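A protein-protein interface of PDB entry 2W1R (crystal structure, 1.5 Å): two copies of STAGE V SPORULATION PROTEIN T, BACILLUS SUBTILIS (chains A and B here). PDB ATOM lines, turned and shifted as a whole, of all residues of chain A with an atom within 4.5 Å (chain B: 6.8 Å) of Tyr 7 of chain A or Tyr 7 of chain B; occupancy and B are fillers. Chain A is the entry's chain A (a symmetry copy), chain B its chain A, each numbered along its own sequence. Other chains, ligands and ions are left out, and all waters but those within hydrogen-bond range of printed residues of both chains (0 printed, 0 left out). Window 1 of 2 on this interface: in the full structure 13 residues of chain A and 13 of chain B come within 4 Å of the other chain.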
ATOM      1  N   PHE A   3      24.677 -13.313 -18.029  1.00  0.00           N
ATOM      2  CA  PHE A   3      23.228 -13.320 -17.864  1.00  0.00           C
ATOM      3  C   PHE A   3      22.490 -14.212 -18.873  1.00  0.00           C
ATOM      4  O   PHE A   3      21.573 -14.960 -18.510  1.00  0.00           O
ATOM      5  CB  PHE A   3      22.722 -11.886 -17.972  1.00  0.00           C
ATOM      6  CG  PHE A   3      21.391 -11.666 -17.340  1.00  0.00           C
ATOM      7  CD1 PHE A   3      21.280 -11.555 -15.960  1.00  0.00           C
ATOM      8  CD2 PHE A   3      20.250 -11.553 -18.120  1.00  0.00           C
ATOM      9  CE1 PHE A   3      20.053 -11.344 -15.368  1.00  0.00           C
ATOM     10  CE2 PHE A   3      19.013 -11.341 -17.534  1.00  0.00           C
ATOM     11  CZ  PHE A   3      18.915 -11.234 -16.152  1.00  0.00           C
ATOM     12  N   ALA A   4      22.888 -14.110 -20.138  1.00  0.00           N
ATOM     13  CA  ALA A   4      22.337 -14.942 -21.200  1.00  0.00           C
ATOM     14  C   ALA A   4      22.689 -16.410 -20.972  1.00  0.00           C
ATOM     15  O   ALA A   4      21.857 -17.291 -21.193  1.00  0.00           O
ATOM     16  CB  ALA A   4      22.840 -14.472 -22.559  1.00  0.00           C
ATOM     17  N   LYS A   5      23.916 -16.662 -20.511  1.00  0.00           N
ATOM     18  CA  LYS A   5      24.373 -18.023 -20.234  1.00  0.00           C
ATOM     19  C   LYS A   5      23.540 -18.674 -19.133  1.00  0.00           C
ATOM     20  O   LYS A   5      23.158 -19.837 -19.247  1.00  0.00           O
ATOM     21  CB  LYS A   5      25.859 -18.040 -19.857  1.00  0.00           C
ATOM     22  CG  LYS A   5      26.443 -19.432 -19.679  1.00  0.00           C
ATOM     23  CD  LYS A   5      27.896 -19.382 -19.229  1.00  0.00           C
ATOM     24  CE  LYS A   5      28.464 -20.785 -19.029  1.00  0.00           C
ATOM     25  NZ  LYS A   5      27.849 -21.497 -17.865  1.00  0.00           N
ATOM     26  N   GLU A   6      23.263 -17.915 -18.073  1.00  0.00           N
ATOM     27  CA  GLU A   6      22.445 -18.396 -16.962  1.00  0.00           C
ATOM     28  C   GLU A   6      21.053 -18.803 -17.437  1.00  0.00           C
ATOM     29  O   GLU A   6      20.547 -19.858 -17.050  1.00  0.00           O
ATOM     30  CB  GLU A   6      22.335 -17.329 -15.869  1.00  0.00           C
ATOM     31  CG  GLU A   6      23.599 -17.148 -15.043  1.00  0.00           C
ATOM     32  CD  GLU A   6      23.668 -15.800 -14.334  1.00  0.00           C
ATOM     33  OE1 GLU A   6      22.610 -15.185 -14.074  1.00  0.00           O
ATOM     34  OE2 GLU A   6      24.796 -15.353 -14.032  1.00  0.00           O
ATOM     35  N   TYR A   7      20.446 -17.970 -18.285  1.00  0.00           N
ATOM     36  CA  TYR A   7      19.102 -18.233 -18.782  1.00  0.00           C
ATOM     37  C   TYR A   7      19.113 -19.448 -19.705  1.00  0.00           C
ATOM     38  O   TYR A   7      18.261 -20.329 -19.584  1.00  0.00           O
ATOM     39  CB  TYR A   7      18.503 -17.011 -19.494  1.00  0.00           C
ATOM     40  CG  TYR A   7      16.993 -16.994 -19.461  1.00  0.00           C
ATOM     41  CD1 TYR A   7      16.299 -15.983 -18.802  1.00  0.00           C
ATOM     42  CD2 TYR A   7      16.250 -18.005 -20.072  1.00  0.00           C
ATOM     43  CE1 TYR A   7      14.906 -15.973 -18.760  1.00  0.00           C
ATOM     44  CE2 TYR A   7      14.860 -18.008 -20.026  1.00  0.00           C
ATOM     45  CZ  TYR A   7      14.195 -16.994 -19.373  1.00  0.00           C
ATOM     46  OH  TYR A   7      12.820 -16.992 -19.338  1.00  0.00           O
ATOM     47  N   ALA A   8      20.092 -19.501 -20.605  1.00  0.00           N
ATOM     48  CA  ALA A   8      20.229 -20.638 -21.505  1.00  0.00           C
ATOM     49  C   ALA A   8      20.373 -21.929 -20.705  1.00  0.00           C
ATOM     50  O   ALA A   8      19.765 -22.938 -21.044  1.00  0.00           O
ATOM     51  CB  ALA A   8      21.413 -20.438 -22.454  1.00  0.00           C
ATOM     52  N   ASP A   9      21.164 -21.886 -19.632  1.00  0.00           N
ATOM     53  CA  ASP A   9      21.347 -23.062 -18.781  1.00  0.00           C
ATOM     54  C   ASP A   9      20.043 -23.471 -18.106  1.00  0.00           C
ATOM     55  O   ASP A   9      19.722 -24.658 -18.025  1.00  0.00           O
ATOM     56  CB  ASP A   9      22.429 -22.811 -17.726  1.00  0.00           C
ATOM     57  CG  ASP A   9      23.836 -22.824 -18.311  1.00  0.00           C
ATOM     58  OD1 ASP A   9      24.024 -23.349 -19.427  1.00  0.00           O
ATOM     59  OD2 ASP A   9      24.761 -22.312 -17.640  1.00  0.00           O
ATOM     60  N   ALA A  10      19.295 -22.480 -17.625  1.00  0.00           N
ATOM     61  CA  ALA A  10      18.001 -22.728 -16.985  1.00  0.00           C
ATOM     62  C   ALA A  10      17.006 -23.340 -17.960  1.00  0.00           C
ATOM     63  O   ALA A  10      16.245 -24.241 -17.602  1.00  0.00           O
ATOM     64  CB  ALA A  10      17.435 -21.451 -16.398  1.00  0.00           C
ATOM     65  N   LEU A  11      17.022 -22.852 -19.197  1.00  0.00           N
ATOM     66  CA  LEU A  11      16.161 -23.401 -20.238  1.00  0.00           C
ATOM     67  C   LEU A  11      16.529 -24.835 -20.582  1.00  0.00           C
ATOM     68  O   LEU A  11      15.652 -25.677 -20.774  1.00  0.00           O
ATOM     69  CB  LEU A  11      16.192 -22.525 -21.489  1.00  0.00           C
ATOM     70  CG  LEU A  11      15.279 -21.303 -21.488  1.00  0.00           C
ATOM     71  CD1 LEU A  11      15.700 -20.371 -22.605  1.00  0.00           C
ATOM     72  CD2 LEU A  11      13.804 -21.702 -21.640  1.00  0.00           C
ATOM     73  N   THR A 112       9.107 -15.807 -23.749  1.00  0.00           N
ATOM     74  CA  THR A 112       9.302 -15.391 -22.368  1.00  0.00           C
ATOM     75  C   THR A 112      10.749 -14.983 -22.117  1.00  0.00           C
ATOM     76  O   THR A 112      11.012 -13.926 -21.532  1.00  0.00           O
ATOM     77  CB  THR A 112       8.902 -16.509 -21.397  1.00  0.00           C
ATOM     78  OG1 THR A 112       7.514 -16.800 -21.570  1.00  0.00           O
ATOM     79  CG2 THR A 112       9.140 -16.070 -19.964  1.00  0.00           C
ATOM     80  N   ALA A 113      11.675 -15.833 -22.559  1.00  0.00           N
ATOM     81  CA  ALA A 113      13.104 -15.570 -22.428  1.00  0.00           C
ATOM     82  C   ALA A 113      13.471 -14.263 -23.109  1.00  0.00           C
ATOM     83  O   ALA A 113      14.151 -13.426 -22.514  1.00  0.00           O
ATOM     84  CB  ALA A 113      13.905 -16.717 -23.016  1.00  0.00           C
ATOM     85  N   PHE A 116      12.139 -11.211 -21.155  1.00  0.00           N
ATOM     86  CA  PHE A 116      12.910 -10.968 -19.948  1.00  0.00           C
ATOM     87  C   PHE A 116      14.295 -10.397 -20.254  1.00  0.00           C
ATOM     88  O   PHE A 116      14.742  -9.447 -19.604  1.00  0.00           O
ATOM     89  CB  PHE A 116      13.035 -12.246 -19.125  1.00  0.00           C
ATOM     90  CG  PHE A 116      13.856 -12.081 -17.890  1.00  0.00           C
ATOM     91  CD1 PHE A 116      13.345 -11.416 -16.779  1.00  0.00           C
ATOM     92  CD2 PHE A 116      15.143 -12.585 -17.834  1.00  0.00           C
ATOM     93  CE1 PHE A 116      14.109 -11.261 -15.634  1.00  0.00           C
ATOM     94  CE2 PHE A 116      15.907 -12.433 -16.695  1.00  0.00           C
ATOM     95  CZ  PHE A 116      15.391 -11.775 -15.590  1.00  0.00           C
ATOM     96  N   LEU A 117      14.964 -10.973 -21.249  1.00  0.00           N
ATOM     97  CA  LEU A 117      16.308 -10.532 -21.625  1.00  0.00           C
ATOM     98  C   LEU A 117      16.311  -9.135 -22.234  1.00  0.00           C
ATOM     99  O   LEU A 117      17.299  -8.407 -22.097  1.00  0.00           O
ATOM    100  CB  LEU A 117      16.973 -11.539 -22.566  1.00  0.00           C
ATOM    101  CG  LEU A 117      17.303 -12.916 -21.975  1.00  0.00           C
ATOM    102  CD1 LEU A 117      17.745 -13.869 -23.066  1.00  0.00           C
ATOM    103  CD2 LEU A 117      18.356 -12.833 -20.864  1.00  0.00           C
ATOM    104  N   ASP B   2      14.442  -4.719  -9.305  1.00  0.00           N
ATOM    105  CA  ASP B   2      13.605  -5.846  -8.794  1.00  0.00           C
ATOM    106  C   ASP B   2      13.586  -7.001  -9.798  1.00  0.00           C
ATOM    107  O   ASP B   2      12.864  -6.973 -10.800  1.00  0.00           O
ATOM    108  CB  ASP B   2      12.189  -5.358  -8.472  1.00  0.00           C
ATOM    109  CG  ASP B   2      11.425  -6.307  -7.552  1.00  0.00           C
ATOM    110  OD1 ASP B   2      11.773  -7.509  -7.474  1.00  0.00           O
ATOM    111  OD2 ASP B   2      10.452  -5.839  -6.914  1.00  0.00           O
ATOM    112  N   PHE B   3      14.381  -8.020  -9.497  1.00  0.00           N
ATOM    113  CA  PHE B   3      14.644  -9.139 -10.395  1.00  0.00           C
ATOM    114  C   PHE B   3      13.448 -10.083 -10.580  1.00  0.00           C
ATOM    115  O   PHE B   3      13.135 -10.502 -11.703  1.00  0.00           O
ATOM    116  CB  PHE B   3      15.841  -9.917  -9.860  1.00  0.00           C
ATOM    117  CG  PHE B   3      16.531 -10.745 -10.888  1.00  0.00           C
ATOM    118  CD1 PHE B   3      17.384 -10.152 -11.809  1.00  0.00           C
ATOM    119  CD2 PHE B   3      16.344 -12.118 -10.928  1.00  0.00           C
ATOM    120  CE1 PHE B   3      18.032 -10.912 -12.760  1.00  0.00           C
ATOM    121  CE2 PHE B   3      16.991 -12.891 -11.879  1.00  0.00           C
ATOM    122  CZ  PHE B   3      17.840 -12.285 -12.797  1.00  0.00           C
ATOM    123  N   ALA B   4      12.799 -10.424  -9.470  1.00  0.00           N
ATOM    124  CA  ALA B   4      11.600 -11.253  -9.489  1.00  0.00           C
ATOM    125  C   ALA B   4      10.459 -10.534 -10.205  1.00  0.00           C
ATOM    126  O   ALA B   4       9.710 -11.155 -10.960  1.00  0.00           O
ATOM    127  CB  ALA B   4      11.193 -11.632  -8.071  1.00  0.00           C
ATOM    128  N   LYS B   5      10.347  -9.224  -9.978  1.00  0.00           N
ATOM    129  CA  LYS B   5       9.308  -8.415 -10.613  1.00  0.00           C
ATOM    130  C   LYS B   5       9.465  -8.405 -12.132  1.00  0.00           C
ATOM    131  O   LYS B   5       8.483  -8.537 -12.860  1.00  0.00           O
ATOM    132  CB  LYS B   5       9.314  -6.982 -10.069  1.00  0.00           C
ATOM    133  CG  LYS B   5       8.180  -6.112 -10.587  1.00  0.00           C
ATOM    134  CD  LYS B   5       8.285  -4.682 -10.074  1.00  0.00           C
ATOM    135  CE  LYS B   5       7.156  -3.813 -10.621  1.00  0.00           C
ATOM    136  NZ  LYS B   5       7.270  -3.576 -12.095  1.00  0.00           N
ATOM    137  N   GLU B   6      10.705  -8.250 -12.597  1.00  0.00           N
ATOM    138  CA  GLU B   6      11.008  -8.259 -14.026  1.00  0.00           C
ATOM    139  C   GLU B   6      10.584  -9.576 -14.673  1.00  0.00           C
ATOM    140  O   GLU B   6       9.979  -9.575 -15.746  1.00  0.00           O
ATOM    141  CB  GLU B   6      12.499  -8.014 -14.266  1.00  0.00           C
ATOM    142  CG  GLU B   6      12.941  -6.576 -14.039  1.00  0.00           C
ATOM    143  CD  GLU B   6      14.437  -6.438 -13.781  1.00  0.00           C
ATOM    144  OE1 GLU B   6      15.220  -7.314 -14.211  1.00  0.00           O
ATOM    145  OE2 GLU B   6      14.833  -5.439 -13.142  1.00  0.00           O
ATOM    146  N   TYR B   7      10.894 -10.691 -14.008  1.00  0.00           N
ATOM    147  CA  TYR B   7      10.572 -12.009 -14.540  1.00  0.00           C
ATOM    148  C   TYR B   7       9.061 -12.219 -14.545  1.00  0.00           C
ATOM    149  O   TYR B   7       8.500 -12.680 -15.538  1.00  0.00           O
ATOM    150  CB  TYR B   7      11.278 -13.130 -13.763  1.00  0.00           C
ATOM    151  CG  TYR B   7      11.497 -14.373 -14.592  1.00  0.00           C
ATOM    152  CD1 TYR B   7      12.781 -14.824 -14.888  1.00  0.00           C
ATOM    153  CD2 TYR B   7      10.417 -15.092 -15.108  1.00  0.00           C
ATOM    154  CE1 TYR B   7      12.984 -15.963 -15.665  1.00  0.00           C
ATOM    155  CE2 TYR B   7      10.613 -16.224 -15.892  1.00  0.00           C
ATOM    156  CZ  TYR B   7      11.891 -16.654 -16.165  1.00  0.00           C
ATOM    157  OH  TYR B   7      12.083 -17.781 -16.932  1.00  0.00           O
ATOM    158  N   ALA B   8       8.409 -11.856 -13.443  1.00  0.00           N
ATOM    159  CA  ALA B   8       6.959 -11.965 -13.353  1.00  0.00           C
ATOM    160  C   ALA B   8       6.300 -11.163 -14.471  1.00  0.00           C
ATOM    161  O   ALA B   8       5.353 -11.630 -15.093  1.00  0.00           O
ATOM    162  CB  ALA B   8       6.465 -11.510 -11.978  1.00  0.00           C
ATOM    163  N   ASP B   9       6.818  -9.963 -14.736  1.00  0.00           N
ATOM    164  CA  ASP B   9       6.278  -9.126 -15.807  1.00  0.00           C
ATOM    165  C   ASP B   9       6.465  -9.778 -17.172  1.00  0.00           C
ATOM    166  O   ASP B   9       5.562  -9.753 -18.010  1.00  0.00           O
ATOM    167  CB  ASP B   9       6.924  -7.736 -15.795  1.00  0.00           C
ATOM    168  CG  ASP B   9       6.422  -6.864 -14.651  1.00  0.00           C
ATOM    169  OD1 ASP B   9       5.358  -7.171 -14.076  1.00  0.00           O
ATOM    170  OD2 ASP B   9       7.096  -5.858 -14.334  1.00  0.00           O
ATOM    171  N   ALA B  10       7.642 -10.361 -17.388  1.00  0.00           N
ATOM    172  CA  ALA B  10       7.943 -11.056 -18.642  1.00  0.00           C
ATOM    173  C   ALA B  10       7.029 -12.256 -18.845  1.00  0.00           C
ATOM    174  O   ALA B  10       6.568 -12.516 -19.959  1.00  0.00           O
ATOM    175  CB  ALA B  10       9.393 -11.494 -18.683  1.00  0.00           C
ATOM    176  N   LEU B  11       6.764 -12.981 -17.762  1.00  0.00           N
ATOM    177  CA  LEU B  11       5.851 -14.117 -17.818  1.00  0.00           C
ATOM    178  C   LEU B  11       4.426 -13.686 -18.126  1.00  0.00           C
ATOM    179  O   LEU B  11       3.731 -14.336 -18.906  1.00  0.00           O
ATOM    180  CB  LEU B  11       5.898 -14.918 -16.518  1.00  0.00           C
ATOM    181  CG  LEU B  11       7.029 -15.934 -16.385  1.00  0.00           C
ATOM    182  CD1 LEU B  11       7.148 -16.353 -14.934  1.00  0.00           C
ATOM    183  CD2 LEU B  11       6.798 -17.154 -17.287  1.00  0.00           C
ATOM    184  N   TYR B  12       3.989 -12.587 -17.510  1.00  0.00           N
ATOM    185  CA  TYR B  12       2.654 -12.073 -17.770  1.00  0.00           C
ATOM    186  C   TYR B  12       2.535 -11.614 -19.215  1.00  0.00           C
ATOM    187  O   TYR B  12       1.580 -11.974 -19.908  1.00  0.00           O
ATOM    188  CB  TYR B  12       2.283 -10.928 -16.823  1.00  0.00           C
ATOM    189  CG  TYR B  12       0.964 -10.285 -17.196  1.00  0.00           C
ATOM    190  CD1 TYR B  12      -0.227 -11.013 -17.126  1.00  0.00           C
ATOM    191  CD2 TYR B  12       0.907  -8.962 -17.632  1.00  0.00           C
ATOM    192  CE1 TYR B  12      -1.444 -10.440 -17.477  1.00  0.00           C
ATOM    193  CE2 TYR B  12      -0.312  -8.375 -17.985  1.00  0.00           C
ATOM    194  CZ  TYR B  12      -1.480  -9.125 -17.900  1.00  0.00           C
ATOM    195  OH  TYR B  12      -2.692  -8.570 -18.242  1.00  0.00           O
ATOM    196  N   ASP B  13       3.515 -10.832 -19.669  1.00  0.00           N
ATOM    197  CA  ASP B  13       3.515 -10.314 -21.040  1.00  0.00           C
ATOM    198  C   ASP B  13       3.435 -11.430 -22.080  1.00  0.00           C
ATOM    199  O   ASP B  13       2.746 -11.295 -23.089  1.00  0.00           O
ATOM    200  CB  ASP B  13       4.767  -9.478 -21.313  1.00  0.00           C
ATOM    201  CG  ASP B  13       4.759  -8.145 -20.590  1.00  0.00           C
ATOM    202  OD1 ASP B  13       3.708  -7.757 -20.034  1.00  0.00           O
ATOM    203  OD2 ASP B  13       5.821  -7.485 -20.585  1.00  0.00           O
ATOM    204  N   VAL B  19       0.738 -13.983 -12.429  1.00  0.00           N
ATOM    205  CA  VAL B  19       1.997 -14.558 -11.991  1.00  0.00           C
ATOM    206  C   VAL B  19       2.313 -14.039 -10.596  1.00  0.00           C
ATOM    207  O   VAL B  19       2.264 -12.830 -10.355  1.00  0.00           O
ATOM    208  CB  VAL B  19       3.155 -14.159 -12.931  1.00  0.00           C
ATOM    209  CG1 VAL B  19       4.455 -14.836 -12.497  1.00  0.00           C
ATOM    210  CG2 VAL B  19       2.837 -14.520 -14.380  1.00  0.00           C
ATOM    211  N   ILE B  21       5.339 -14.487  -7.458  1.00  0.00           N
ATOM    212  CA  ILE B  21       6.591 -15.050  -6.984  1.00  0.00           C
ATOM    213  C   ILE B  21       6.653 -14.784  -5.496  1.00  0.00           C
ATOM    214  O   ILE B  21       6.394 -13.668  -5.052  1.00  0.00           O
ATOM    215  CB  ILE B  21       7.823 -14.473  -7.718  1.00  0.00           C
ATOM    216  CG1 ILE B  21       7.707 -14.780  -9.222  1.00  0.00           C
ATOM    217  CG2 ILE B  21       9.110 -15.063  -7.142  1.00  0.00           C
ATOM    218  CD1 ILE B  21       8.816 -14.219 -10.095  1.00  0.00           C
ATOM    219  N   SER B  31       2.274 -10.006 -10.999  1.00  0.00           N
ATOM    220  CA  SER B  31       1.997  -9.460 -12.324  1.00  0.00           C
ATOM    221  C   SER B  31       0.679 -10.009 -12.836  1.00  0.00           C
ATOM    222  O   SER B  31       0.338 -11.159 -12.567  1.00  0.00           O
ATOM    223  CB  SER B  31       3.132  -9.781 -13.289  1.00  0.00           C
ATOM    224  OG  SER B  31       4.347  -9.249 -12.804  1.00  0.00           O
ATOM    225  N   VAL B  93       7.440 -19.884  -7.887  1.00  0.00           N
ATOM    226  CA  VAL B  93       6.822 -19.139  -8.965  1.00  0.00           C
ATOM    227  C   VAL B  93       5.465 -19.784  -9.204  1.00  0.00           C
ATOM    228  O   VAL B  93       5.363 -21.011  -9.319  1.00  0.00           O
ATOM    229  CB  VAL B  93       7.672 -19.196 -10.250  1.00  0.00           C
ATOM    230  CG1 VAL B  93       7.013 -18.399 -11.371  1.00  0.00           C
ATOM    231  CG2 VAL B  93       9.086 -18.673  -9.995  1.00  0.00           C
ATOM    232  N   ALA B 109       7.031 -23.251 -17.732  1.00  0.00           N
ATOM    233  CA  ALA B 109       7.402 -21.857 -17.485  1.00  0.00           C
ATOM    234  C   ALA B 109       7.775 -21.637 -16.022  1.00  0.00           C
ATOM    235  O   ALA B 109       8.777 -20.982 -15.736  1.00  0.00           O
ATOM    236  CB  ALA B 109       6.292 -20.911 -17.898  1.00  0.00           C
ATOM    237  N   GLU B 111       8.834 -23.911 -13.897  1.00  0.00           N
ATOM    238  CA  GLU B 111      10.059 -24.656 -13.633  1.00  0.00           C
ATOM    239  C   GLU B 111      11.264 -23.893 -14.174  1.00  0.00           C
ATOM    240  O   GLU B 111      12.271 -23.754 -13.487  1.00  0.00           O
ATOM    241  CB  GLU B 111       9.998 -26.063 -14.223  1.00  0.00           C
ATOM    242  CG  GLU B 111      11.217 -26.905 -13.868  1.00  0.00           C
ATOM    243  CD  GLU B 111      11.247 -28.248 -14.561  1.00  0.00           C
ATOM    244  OE1 GLU B 111      10.174 -28.746 -14.962  1.00  0.00           O
ATOM    245  OE2 GLU B 111      12.355 -28.814 -14.697  1.00  0.00           O
ATOM    246  N   THR B 112      11.142 -23.384 -15.396  1.00  0.00           N
ATOM    247  CA  THR B 112      12.211 -22.600 -15.996  1.00  0.00           C
ATOM    248  C   THR B 112      12.506 -21.353 -15.170  1.00  0.00           C
ATOM    249  O   THR B 112      13.670 -21.057 -14.874  1.00  0.00           O
ATOM    250  CB  THR B 112      11.856 -22.199 -17.433  1.00  0.00           C
ATOM    251  OG1 THR B 112      11.692 -23.382 -18.219  1.00  0.00           O
ATOM    252  CG2 THR B 112      12.967 -21.357 -18.033  1.00  0.00           C
ATOM    253  N   ALA B 113      11.446 -20.632 -14.812  1.00  0.00           N
ATOM    254  CA  ALA B 113      11.558 -19.431 -13.990  1.00  0.00           C
ATOM    255  C   ALA B 113      12.231 -19.751 -12.667  1.00  0.00           C
ATOM    256  O   ALA B 113      13.165 -19.055 -12.265  1.00  0.00           O
ATOM    257  CB  ALA B 113      10.187 -18.825 -13.755  1.00  0.00           C
ATOM    258  N   ALA B 114      11.760 -20.805 -12.003  1.00  0.00           N
ATOM    259  CA  ALA B 114      12.319 -21.206 -10.710  1.00  0.00           C
ATOM    260  C   ALA B 114      13.802 -21.550 -10.826  1.00  0.00           C
ATOM    261  O   ALA B 114      14.597 -21.174  -9.963  1.00  0.00           O
ATOM    262  CB  ALA B 114      11.547 -22.364 -10.123  1.00  0.00           C
ATOM    263  N   PHE B 116      15.992 -20.496 -13.121  1.00  0.00           N
ATOM    264  CA  PHE B 116      16.752 -19.286 -13.382  1.00  0.00           C
ATOM    265  C   PHE B 116      16.890 -18.411 -12.135  1.00  0.00           C
ATOM    266  O   PHE B 116      17.976 -17.906 -11.838  1.00  0.00           O
ATOM    267  CB  PHE B 116      16.119 -18.491 -14.519  1.00  0.00           C
ATOM    268  CG  PHE B 116      16.822 -17.208 -14.812  1.00  0.00           C
ATOM    269  CD1 PHE B 116      18.040 -17.202 -15.486  1.00  0.00           C
ATOM    270  CD2 PHE B 116      16.274 -16.003 -14.412  1.00  0.00           C
ATOM    271  CE1 PHE B 116      18.694 -16.010 -15.756  1.00  0.00           C
ATOM    272  CE2 PHE B 116      16.922 -14.814 -14.679  1.00  0.00           C
ATOM    273  CZ  PHE B 116      18.131 -14.814 -15.355  1.00  0.00           C
ATOM    274  N   LEU B 117      15.789 -18.245 -11.408  1.00  0.00           N
ATOM    275  CA  LEU B 117      15.785 -17.413 -10.203  1.00  0.00           C
ATOM    276  C   LEU B 117      16.618 -18.017  -9.078  1.00  0.00           C
ATOM    277  O   LEU B 117      17.175 -17.279  -8.260  1.00  0.00           O
ATOM    278  CB  LEU B 117      14.356 -17.132  -9.734  1.00  0.00           C
ATOM    279  CG  LEU B 117      13.490 -16.264 -10.657  1.00  0.00           C
ATOM    280  CD1 LEU B 117      12.052 -16.257 -10.181  1.00  0.00           C
ATOM    281  CD2 LEU B 117      14.030 -14.834 -10.783  1.00  0.00           C
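The side-chain hydroxyl (OH) of Tyr 7 of chain B lies within hydrogen-bond range of the side-chain hydroxyl (OH) of Tyr 7 of chain A, 2.6 Å away.
Among the printed residues, merely in contact across the chains: Phe 116 of chain A with Phe 116 of chain B (3.3 Å), Phe 3 of chain A with Phe 3 of chain B (3.3 Å), Phe 116 of chain A with Tyr 7 of chain B (3.6 Å), Tyr 7 of chain A with Phe 116 of chain B (3.6 Å), Phe 116 of chain A with Ala 10 of chain B (3.7 Å), Ala 10 of chain A with Phe 116 of chain B (3.7 Å), Thr 112 of chain A with Leu 11 of chain B (3.7 Å), Leu 11 of chain A with Thr 112 of chain B (3.7 Å), Phe 116 of chain A with Phe 3 of chain B (3.7 Å), Phe 3 of chain A with Phe 116 of chain B (3.8 Å), Phe 116 of chain A with Glu 6 of chain B (3.9 Å) and Glu 6 of chain A with Phe 116 of chain B (3.9 Å).
Tyr 7 of chain A touches two residues of chain B. Tyr 7 of chain B touches just these residues of chain A: Tyr 7 (2.6 Å) and Phe 116 (3.6 Å). Of the printed residues of chain A, Leu 11 of chain B touches Thr 112 (3.7 Å). Of the printed residues of chain A, Glu 6 of chain B touches Phe 116 (3.9 Å). Ser 31 of chain B touches none of the printed residues of chain A. Ala 113 of chain B touches none of the printed residues of chain A. The nearest residue of chain B that does not touch Tyr 7 of chain A is Thr 112 of chain B (4.3 Å).
Hydrophobic or aromatic side chains of chain A that line the printed part of chain B: Phe 3, Tyr 7, Ala 10, Leu 11 and Phe 116. Among the printed residues, 13 pairs touch across the chains.
Phe 3 of chain B touches its own counterpart, Phe 3 of chain A. Ala 10 of chain A touches Phe 116 of chain B, and with the chains exchanged Phe 116 of chain A touches Ala 10 of chain B. Leu 11 of chain A touches Thr 112 of chain B, and with the chains exchanged Thr 112 of chain A touches Leu 11 of chain B. Phe 116 of chain B touches its own counterpart, Phe 116 of chain A. 13 positions are printed for both chains. Of the 13 pairs that touch across the chains among the printed residues, 13 have their exchanged pair printed and touching as well.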
